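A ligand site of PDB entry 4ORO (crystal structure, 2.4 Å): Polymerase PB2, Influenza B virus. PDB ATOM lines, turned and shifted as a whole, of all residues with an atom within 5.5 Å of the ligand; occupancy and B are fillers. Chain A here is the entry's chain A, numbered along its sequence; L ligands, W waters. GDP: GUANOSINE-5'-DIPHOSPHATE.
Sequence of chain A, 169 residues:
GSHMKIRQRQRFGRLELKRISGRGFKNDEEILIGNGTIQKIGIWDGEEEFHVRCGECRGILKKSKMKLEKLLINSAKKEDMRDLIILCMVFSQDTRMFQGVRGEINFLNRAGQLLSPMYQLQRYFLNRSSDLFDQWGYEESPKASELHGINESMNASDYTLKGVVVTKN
The backbone NH of Met 4 is in hydrogen-bond range of an oxygen (O6) of the ligand, 3.1 Å away.
O4' of the ligand is in hydrogen-bond range of NE1 of Trp 44 (2.9 Å).
An oxygen (O1A) of the ligand sits at hydrogen-bond distance from the side-chain hydroxyl (OG) of Ser 116.
An oxygen (O3B) of the ligand is in salt-bridge range of the side-chain amino group (NZ) of Lys 26 (2.5 Å).
OE1 of Glu 48 lies within hydrogen-bond range of N2 of the ligand, 2.6 Å away.
The guanidinium group (NH2) of Arg 19 lies within hydrogen-bond range of an oxygen (O6) of the ligand (3.2 Å).
The side-chain sulfur (SD) of Met 118 sits at hydrogen-bond distance from the side-chain amide nitrogen (NE2) of Gln 93 (3.3 Å).
The backbone NH (N) of Trp 44 sits at hydrogen-bond distance from the side-chain amide oxygen (OE1) of Gln 93.
OE2 of Glu 48 is in hydrogen-bond range of N of Gly 24 (3.5 Å).
The side-chain carboxylate of Glu 48 is in salt-bridge range of the guanidinium group of Arg 19.
NE of Arg 19 is in hydrogen-bond range of O of Met 4 (2.7 Å).
O of Glu 48 is in hydrogen-bond range of N of Lys 63 (3.1 Å).
Ser 2 touches the ligand.
His 3 touches the ligand (CA to O6, 3.9 Å).
CE1 of Phe 12 touches O3' of the ligand (3.6 Å).
CD of Lys 63 touches N2 of the ligand, at 3.9 Å.
Phe 91 touches the ligand (CZ to N3, 3.3 Å).
Met 118 touches the ligand (CB to O3', 3.4 Å).
Hydrophobic or aromatic side chains that line the ligand: Met 4, Phe 12, Trp 44, Phe 91 and Met 118.
Within 4 Å of the ligand: Ser 2, His 3, Met 4, Phe 12, Arg 19, Lys 26, Trp 44, Glu 48, Lys 63, Phe 91, Ser 116 and Met 118.
Water W6 lies within hydrogen-bond range of an oxygen (O3B) of the ligand and the backbone carbonyl oxygen (O) of Gly 42.
Water W7 bridges an oxygen (O1A) of the ligand and the backbone NH (N) of Met 118.
Water W5 bridges an oxygen (O1B) of the ligand (2.6 Å) and the backbone NH of Gly 42 (3.1 Å).
Water W3 bridges a nitrogen (N3) of the ligand (2.7 Å) and the backbone carbonyl oxygen (O) of Phe 91 (3.2 Å).
Water W1 lies within hydrogen-bond range of an oxygen (O6) of the ligand (2.7 Å), the backbone NH (N) of Gly 24 (3.0 Å) and the guanidinium group (NH2) of Arg 19 (3.4 Å).
Water W8 lies within hydrogen-bond range of O of Arg 11 (2.6 Å) and O2' of the ligand (2.9 Å).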
ATOM      1  N   GLY A   1      15.981  -2.417  17.927  1.00  0.00           N
ATOM      2  CA  GLY A   1      15.827  -3.887  18.080  1.00  0.00           C
ATOM      3  C   GLY A   1      16.376  -4.394  19.397  1.00  0.00           C
ATOM      4  O   GLY A   1      16.441  -3.642  20.414  1.00  0.00           O
ATOM      5  N   SER A   2      16.794  -5.662  19.334  1.00  0.00           N
ATOM      6  CA  SER A   2      17.250  -6.467  20.474  1.00  0.00           C
ATOM      7  C   SER A   2      18.706  -6.221  20.860  1.00  0.00           C
ATOM      8  O   SER A   2      19.071  -6.343  22.040  1.00  0.00           O
ATOM      9  CB  SER A   2      17.132  -7.965  20.146  1.00  0.00           C
ATOM     10  OG  SER A   2      15.990  -8.239  19.344  1.00  0.00           O
ATOM     11  N   HIS A   3      19.529  -5.959  19.858  1.00  0.00           N
ATOM     12  CA  HIS A   3      20.965  -5.797  20.010  1.00  0.00           C
ATOM     13  C   HIS A   3      21.488  -4.664  19.081  1.00  0.00           C
ATOM     14  O   HIS A   3      20.978  -4.444  18.000  1.00  0.00           O
ATOM     15  CB  HIS A   3      21.733  -7.155  19.923  1.00  0.00           C
ATOM     16  CG  HIS A   3      21.710  -7.814  18.559  1.00  0.00           C
ATOM     17  ND1 HIS A   3      20.565  -8.318  17.979  1.00  0.00           N
ATOM     18  CD2 HIS A   3      22.721  -8.059  17.674  1.00  0.00           C
ATOM     19  CE1 HIS A   3      20.858  -8.816  16.781  1.00  0.00           C
ATOM     20  NE2 HIS A   3      22.153  -8.687  16.584  1.00  0.00           N
ATOM     21  N   MET A   4      22.442  -3.899  19.553  1.00  0.00           N
ATOM     22  CA  MET A   4      22.982  -2.831  18.759  1.00  0.00           C
ATOM     23  C   MET A   4      24.043  -3.319  17.787  1.00  0.00           C
ATOM     24  O   MET A   4      25.063  -3.888  18.173  1.00  0.00           O
ATOM     25  CB  MET A   4      23.561  -1.746  19.662  1.00  0.00           C
ATOM     26  CG  MET A   4      22.492  -0.823  20.212  1.00  0.00           C
ATOM     27  SD  MET A   4      23.142   0.062  21.638  1.00  0.00           S
ATOM     28  CE  MET A   4      21.573   0.711  22.284  1.00  0.00           C
ATOM     29  N   ARG A  11      19.810   4.588  19.989  1.00  0.00           N
ATOM     30  CA  ARG A  11      19.398   5.463  21.090  1.00  0.00           C
ATOM     31  C   ARG A  11      19.034   4.730  22.443  1.00  0.00           C
ATOM     32  O   ARG A  11      18.385   3.654  22.469  1.00  0.00           O
ATOM     33  CB  ARG A  11      18.190   6.364  20.656  1.00  0.00           C
ATOM     34  CG  ARG A  11      18.424   7.384  19.505  1.00  0.00           C
ATOM     35  CD  ARG A  11      19.567   8.417  19.752  1.00  0.00           C
ATOM     36  NE  ARG A  11      19.474   9.271  20.947  1.00  0.00           N
ATOM     37  CZ  ARG A  11      19.544  10.621  20.966  1.00  0.00           C
ATOM     38  NH1 ARG A  11      19.648  11.350  19.847  1.00  0.00           N
ATOM     39  NH2 ARG A  11      19.480  11.268  22.137  1.00  0.00           N
ATOM     40  N   PHE A  12      19.440   5.336  23.557  1.00  0.00           N
ATOM     41  CA  PHE A  12      19.007   4.980  24.890  1.00  0.00           C
ATOM     42  C   PHE A  12      18.679   6.352  25.479  1.00  0.00           C
ATOM     43  O   PHE A  12      19.539   6.965  26.179  1.00  0.00           O
ATOM     44  CB  PHE A  12      20.173   4.303  25.628  1.00  0.00           C
ATOM     45  CG  PHE A  12      19.955   4.141  27.099  1.00  0.00           C
ATOM     46  CD1 PHE A  12      18.731   3.784  27.587  1.00  0.00           C
ATOM     47  CD2 PHE A  12      21.009   4.309  27.999  1.00  0.00           C
ATOM     48  CE1 PHE A  12      18.533   3.623  28.947  1.00  0.00           C
ATOM     49  CE2 PHE A  12      20.816   4.137  29.372  1.00  0.00           C
ATOM     50  CZ  PHE A  12      19.570   3.796  29.835  1.00  0.00           C
ATOM     51  N   ARG A  19      28.127   1.129  17.753  1.00  0.00           N
ATOM     52  CA  ARG A  19      29.035   0.065  18.044  1.00  0.00           C
ATOM     53  C   ARG A  19      30.321   0.042  17.258  1.00  0.00           C
ATOM     54  O   ARG A  19      30.289   0.074  16.085  1.00  0.00           O
ATOM     55  CB  ARG A  19      28.362  -1.296  17.951  1.00  0.00           C
ATOM     56  CG  ARG A  19      29.324  -2.409  18.266  1.00  0.00           C
ATOM     57  CD  ARG A  19      28.815  -3.734  17.993  1.00  0.00           C
ATOM     58  NE  ARG A  19      27.650  -4.026  18.754  1.00  0.00           N
ATOM     59  CZ  ARG A  19      27.659  -4.187  20.038  1.00  0.00           C
ATOM     60  NH1 ARG A  19      28.765  -4.089  20.702  1.00  0.00           N
ATOM     61  NH2 ARG A  19      26.558  -4.403  20.652  1.00  0.00           N
ATOM     62  N   GLY A  24      27.170  -8.200  23.105  1.00  0.00           N
ATOM     63  CA  GLY A  24      26.568  -8.476  24.404  1.00  0.00           C
ATOM     64  C   GLY A  24      25.569  -9.629  24.317  1.00  0.00           C
ATOM     65  O   GLY A  24      24.934  -9.808  23.277  1.00  0.00           O
ATOM     66  N   LYS A  26      22.215 -10.652  26.713  1.00  0.00           N
ATOM     67  CA  LYS A  26      21.423 -10.183  27.823  1.00  0.00           C
ATOM     68  C   LYS A  26      20.773 -11.362  28.602  1.00  0.00           C
ATOM     69  O   LYS A  26      20.279 -12.273  27.976  1.00  0.00           O
ATOM     70  CB  LYS A  26      20.385  -9.218  27.288  1.00  0.00           C
ATOM     71  CG  LYS A  26      19.506  -8.626  28.346  1.00  0.00           C
ATOM     72  CD  LYS A  26      18.640  -7.515  27.859  1.00  0.00           C
ATOM     73  CE  LYS A  26      17.720  -7.948  26.774  1.00  0.00           C
ATOM     74  NZ  LYS A  26      16.477  -7.166  26.949  1.00  0.00           N
ATOM     75  N   ASP A  28      18.210 -11.961  32.242  1.00  0.00           N
ATOM     76  CA  ASP A  28      17.540 -11.357  33.416  1.00  0.00           C
ATOM     77  C   ASP A  28      18.178 -11.789  34.742  1.00  0.00           C
ATOM     78  O   ASP A  28      18.523 -12.965  34.960  1.00  0.00           O
ATOM     79  CB  ASP A  28      16.020 -11.593  33.459  1.00  0.00           C
ATOM     80  CG  ASP A  28      15.217 -10.521  32.670  1.00  0.00           C
ATOM     81  OD1 ASP A  28      15.697 -10.029  31.627  1.00  0.00           O
ATOM     82  OD2 ASP A  28      14.052 -10.202  33.064  1.00  0.00           O
ATOM     83  N   GLY A  42      17.476  -6.680  32.754  1.00  0.00           N
ATOM     84  CA  GLY A  42      18.237  -7.336  31.691  1.00  0.00           C
ATOM     85  C   GLY A  42      19.701  -6.908  31.732  1.00  0.00           C
ATOM     86  O   GLY A  42      20.043  -5.808  31.316  1.00  0.00           O
ATOM     87  N   TRP A  44      23.453  -7.226  30.476  1.00  0.00           N
ATOM     88  CA  TRP A  44      24.285  -7.564  29.339  1.00  0.00           C
ATOM     89  C   TRP A  44      25.610  -8.111  29.861  1.00  0.00           C
ATOM     90  O   TRP A  44      26.105  -7.635  30.886  1.00  0.00           O
ATOM     91  CB  TRP A  44      24.547  -6.285  28.465  1.00  0.00           C
ATOM     92  CG  TRP A  44      23.311  -5.896  27.796  1.00  0.00           C
ATOM     93  CD1 TRP A  44      22.361  -5.048  28.262  1.00  0.00           C
ATOM     94  CD2 TRP A  44      22.830  -6.393  26.542  1.00  0.00           C
ATOM     95  NE1 TRP A  44      21.316  -4.972  27.363  1.00  0.00           N
ATOM     96  CE2 TRP A  44      21.573  -5.805  26.308  1.00  0.00           C
ATOM     97  CE3 TRP A  44      23.342  -7.278  25.579  1.00  0.00           C
ATOM     98  CZ2 TRP A  44      20.818  -6.069  25.174  1.00  0.00           C
ATOM     99  CZ3 TRP A  44      22.604  -7.547  24.459  1.00  0.00           C
ATOM    100  CH2 TRP A  44      21.351  -6.935  24.251  1.00  0.00           C
ATOM    101  N   GLU A  48      32.082  -4.832  25.121  1.00  0.00           N
ATOM    102  CA  GLU A  48      31.470  -4.007  24.111  1.00  0.00           C
ATOM    103  C   GLU A  48      32.179  -2.653  23.995  1.00  0.00           C
ATOM    104  O   GLU A  48      32.581  -2.127  24.969  1.00  0.00           O
ATOM    105  CB  GLU A  48      29.985  -3.835  24.448  1.00  0.00           C
ATOM    106  CG  GLU A  48      29.212  -5.117  24.524  1.00  0.00           C
ATOM    107  CD  GLU A  48      27.733  -4.900  24.619  1.00  0.00           C
ATOM    108  OE1 GLU A  48      27.234  -4.863  25.715  1.00  0.00           O
ATOM    109  OE2 GLU A  48      27.069  -4.774  23.616  1.00  0.00           O
ATOM    110  N   PHE A  50      31.705   1.216  22.210  1.00  0.00           N
ATOM    111  CA  PHE A  50      30.849   2.132  21.471  1.00  0.00           C
ATOM    112  C   PHE A  50      31.371   3.539  21.303  1.00  0.00           C
ATOM    113  O   PHE A  50      31.993   4.076  22.159  1.00  0.00           O
ATOM    114  CB  PHE A  50      29.499   2.284  22.145  1.00  0.00           C
ATOM    115  CG  PHE A  50      28.722   1.060  22.241  1.00  0.00           C
ATOM    116  CD1 PHE A  50      27.763   0.758  21.324  1.00  0.00           C
ATOM    117  CD2 PHE A  50      28.887   0.233  23.288  1.00  0.00           C
ATOM    118  CE1 PHE A  50      27.042  -0.356  21.439  1.00  0.00           C
ATOM    119  CE2 PHE A  50      28.186  -0.858  23.392  1.00  0.00           C
ATOM    120  CZ  PHE A  50      27.231  -1.150  22.473  1.00  0.00           C
ATOM    121  N   LYS A  63      32.801  -1.346  27.962  1.00  0.00           N
ATOM    122  CA  LYS A  63      32.190  -1.955  29.141  1.00  0.00           C
ATOM    123  C   LYS A  63      32.445  -3.450  29.186  1.00  0.00           C
ATOM    124  O   LYS A  63      32.791  -4.064  28.177  1.00  0.00           O
ATOM    125  CB  LYS A  63      30.680  -1.663  29.138  1.00  0.00           C
ATOM    126  CG  LYS A  63      29.849  -2.548  28.231  1.00  0.00           C
ATOM    127  CD  LYS A  63      28.359  -2.200  28.406  1.00  0.00           C
ATOM    128  CE  LYS A  63      27.664  -2.882  29.607  1.00  0.00           C
ATOM    129  NZ  LYS A  63      28.004  -4.306  29.794  1.00  0.00           N
ATOM    130  N   PHE A  91      24.240   3.228  31.310  1.00  0.00           N
ATOM    131  CA  PHE A  91      24.329   2.291  30.210  1.00  0.00           C
ATOM    132  C   PHE A  91      25.204   1.113  30.525  1.00  0.00           C
ATOM    133  O   PHE A  91      24.888   0.008  30.087  1.00  0.00           O
ATOM    134  CB  PHE A  91      24.864   2.891  28.901  1.00  0.00           C
ATOM    135  CG  PHE A  91      24.781   1.943  27.720  1.00  0.00           C
ATOM    136  CD1 PHE A  91      23.539   1.696  27.105  1.00  0.00           C
ATOM    137  CD2 PHE A  91      25.925   1.300  27.234  1.00  0.00           C
ATOM    138  CE1 PHE A  91      23.450   0.836  26.011  1.00  0.00           C
ATOM    139  CE2 PHE A  91      25.860   0.421  26.147  1.00  0.00           C
ATOM    140  CZ  PHE A  91      24.623   0.182  25.521  1.00  0.00           C
ATOM    141  N   GLN A  93      25.667  -0.368  33.393  1.00  0.00           N
ATOM    142  CA  GLN A  93      25.078  -1.253  34.396  1.00  0.00           C
ATOM    143  C   GLN A  93      26.088  -1.552  35.471  1.00  0.00           C
ATOM    144  O   GLN A  93      26.148  -2.642  36.058  1.00  0.00           O
ATOM    145  CB  GLN A  93      24.507  -2.526  33.739  1.00  0.00           C
ATOM    146  CG  GLN A  93      23.436  -2.214  32.665  1.00  0.00           C
ATOM    147  CD  GLN A  93      22.842  -3.480  32.086  1.00  0.00           C
ATOM    148  OE1 GLN A  93      23.575  -4.408  31.719  1.00  0.00           O
ATOM    149  NE2 GLN A  93      21.497  -3.546  32.031  1.00  0.00           N
ATOM    150  N   SER A 116      10.289   0.851  31.707  1.00  0.00           N
ATOM    151  CA  SER A 116      11.585   0.238  31.501  1.00  0.00           C
ATOM    152  C   SER A 116      12.546   0.550  32.601  1.00  0.00           C
ATOM    153  O   SER A 116      12.812   1.663  32.858  1.00  0.00           O
ATOM    154  CB  SER A 116      12.178   0.700  30.201  1.00  0.00           C
ATOM    155  OG  SER A 116      13.490   0.293  30.065  1.00  0.00           O
ATOM    156  N   PRO A 117      13.062  -0.479  33.225  1.00  0.00           N
ATOM    157  CA  PRO A 117      14.010  -0.317  34.286  1.00  0.00           C
ATOM    158  C   PRO A 117      15.225   0.476  33.918  1.00  0.00           C
ATOM    159  O   PRO A 117      15.513   1.366  34.624  1.00  0.00           O
ATOM    160  CB  PRO A 117      14.349  -1.754  34.629  1.00  0.00           C
ATOM    161  CG  PRO A 117      13.264  -2.409  34.316  1.00  0.00           C
ATOM    162  CD  PRO A 117      12.637  -1.852  33.165  1.00  0.00           C
ATOM    163  N   MET A 118      15.871   0.179  32.813  1.00  0.00           N
ATOM    164  CA  MET A 118      17.083   0.907  32.516  1.00  0.00           C
ATOM    165  C   MET A 118      16.776   2.404  32.229  1.00  0.00           C
ATOM    166  O   MET A 118      17.528   3.303  32.654  1.00  0.00           O
ATOM    167  CB  MET A 118      17.839   0.215  31.408  1.00  0.00           C
ATOM    168  CG  MET A 118      18.466  -1.052  31.912  1.00  0.00           C
ATOM    169  SD  MET A 118      19.869  -0.815  33.038  1.00  0.00           S
ATOM    170  CE  MET A 118      20.834   0.238  32.004  1.00  0.00           C
ATOM    171  N   TYR A 119      15.629   2.654  31.575  1.00  0.00           N
ATOM    172  CA  TYR A 119      15.162   4.026  31.278  1.00  0.00           C
ATOM    173  C   TYR A 119      14.826   4.825  32.523  1.00  0.00           C
ATOM    174  O   TYR A 119      15.155   6.016  32.642  1.00  0.00           O
ATOM    175  CB  TYR A 119      13.894   4.044  30.371  1.00  0.00           C
ATOM    176  CG  TYR A 119      13.730   5.363  29.672  1.00  0.00           C
ATOM    177  CD1 TYR A 119      14.676   5.770  28.742  1.00  0.00           C
ATOM    178  CD2 TYR A 119      12.670   6.243  29.975  1.00  0.00           C
ATOM    179  CE1 TYR A 119      14.580   6.986  28.119  1.00  0.00           C
ATOM    180  CE2 TYR A 119      12.552   7.475  29.327  1.00  0.00           C
ATOM    181  CZ  TYR A 119      13.519   7.841  28.386  1.00  0.00           C
ATOM    182  OH  TYR A 119      13.475   9.040  27.681  1.00  0.00           O
HETATM  183  PB  GDP L   1      14.372  -5.166  28.345  1.00  0.00           P
HETATM  184  O1B GDP L   1      13.479  -5.105  29.582  1.00  0.00           O
HETATM  185  O2B GDP L   1      13.751  -6.132  27.315  1.00  0.00           O
HETATM  186  O3B GDP L   1      15.810  -5.490  28.742  1.00  0.00           O
HETATM  187  O3A GDP L   1      14.386  -3.826  27.481  1.00  0.00           O
HETATM  188  PA  GDP L   1      14.847  -2.422  27.989  1.00  0.00           P
HETATM  189  O1A GDP L   1      14.143  -1.918  29.217  1.00  0.00           O
HETATM  190  O2A GDP L   1      14.649  -1.700  26.690  1.00  0.00           O
HETATM  191  O5' GDP L   1      16.390  -2.666  28.315  1.00  0.00           O
HETATM  192  C5' GDP L   1      17.268  -2.791  27.210  1.00  0.00           C
HETATM  193  C4' GDP L   1      18.536  -2.053  27.623  1.00  0.00           C
HETATM  194  O4' GDP L   1      19.669  -2.645  26.995  1.00  0.00           O
HETATM  195  C3' GDP L   1      18.468  -0.600  27.179  1.00  0.00           C
HETATM  196  O3' GDP L   1      19.078   0.178  28.209  1.00  0.00           O
HETATM  197  C2' GDP L   1      19.330  -0.562  25.953  1.00  0.00           C
HETATM  198  O2' GDP L   1      19.979   0.701  25.692  1.00  0.00           O
HETATM  199  C1' GDP L   1      20.322  -1.636  26.235  1.00  0.00           C
HETATM  200  N9  GDP L   1      20.797  -2.270  25.011  1.00  0.00           N
HETATM  201  C8  GDP L   1      20.149  -2.506  23.815  1.00  0.00           C
HETATM  202  N7  GDP L   1      21.014  -3.153  22.968  1.00  0.00           N
HETATM  203  C5  GDP L   1      22.220  -3.303  23.665  1.00  0.00           C
HETATM  204  C6  GDP L   1      23.559  -3.884  23.408  1.00  0.00           C
HETATM  205  O6  GDP L   1      23.840  -4.419  22.316  1.00  0.00           O
HETATM  206  N1  GDP L   1      24.495  -3.850  24.346  1.00  0.00           N
HETATM  207  C2  GDP L   1      24.263  -3.312  25.525  1.00  0.00           C
HETATM  208  N2  GDP L   1      25.266  -3.378  26.377  1.00  0.00           N
HETATM  209  N3  GDP L   1      23.065  -2.757  25.906  1.00  0.00           N
HETATM  210  C4  GDP L   1      22.054  -2.718  24.987  1.00  0.00           C
HETATM  211  O   HOH W   1      24.687  -6.982  21.908  1.00  0.00           O
HETATM  212  O   HOH W   2      15.430   1.247  27.279  1.00  0.00           O
HETATM  213  O   HOH W   3      23.003  -2.071  28.491  1.00  0.00           O
HETATM  214  O   HOH W   4      11.400  -4.773  26.366  1.00  0.00           O
HETATM  215  O   HOH W   5      14.894  -5.279  31.800  1.00  0.00           O
HETATM  216  O   HOH W   6      17.658  -4.397  30.242  1.00  0.00           O
HETATM  217  O   HOH W   7      15.707  -2.358  31.283  1.00  0.00           O
HETATM  218  O   HOH W   8      18.109   1.345  23.574  1.00  0.00           O
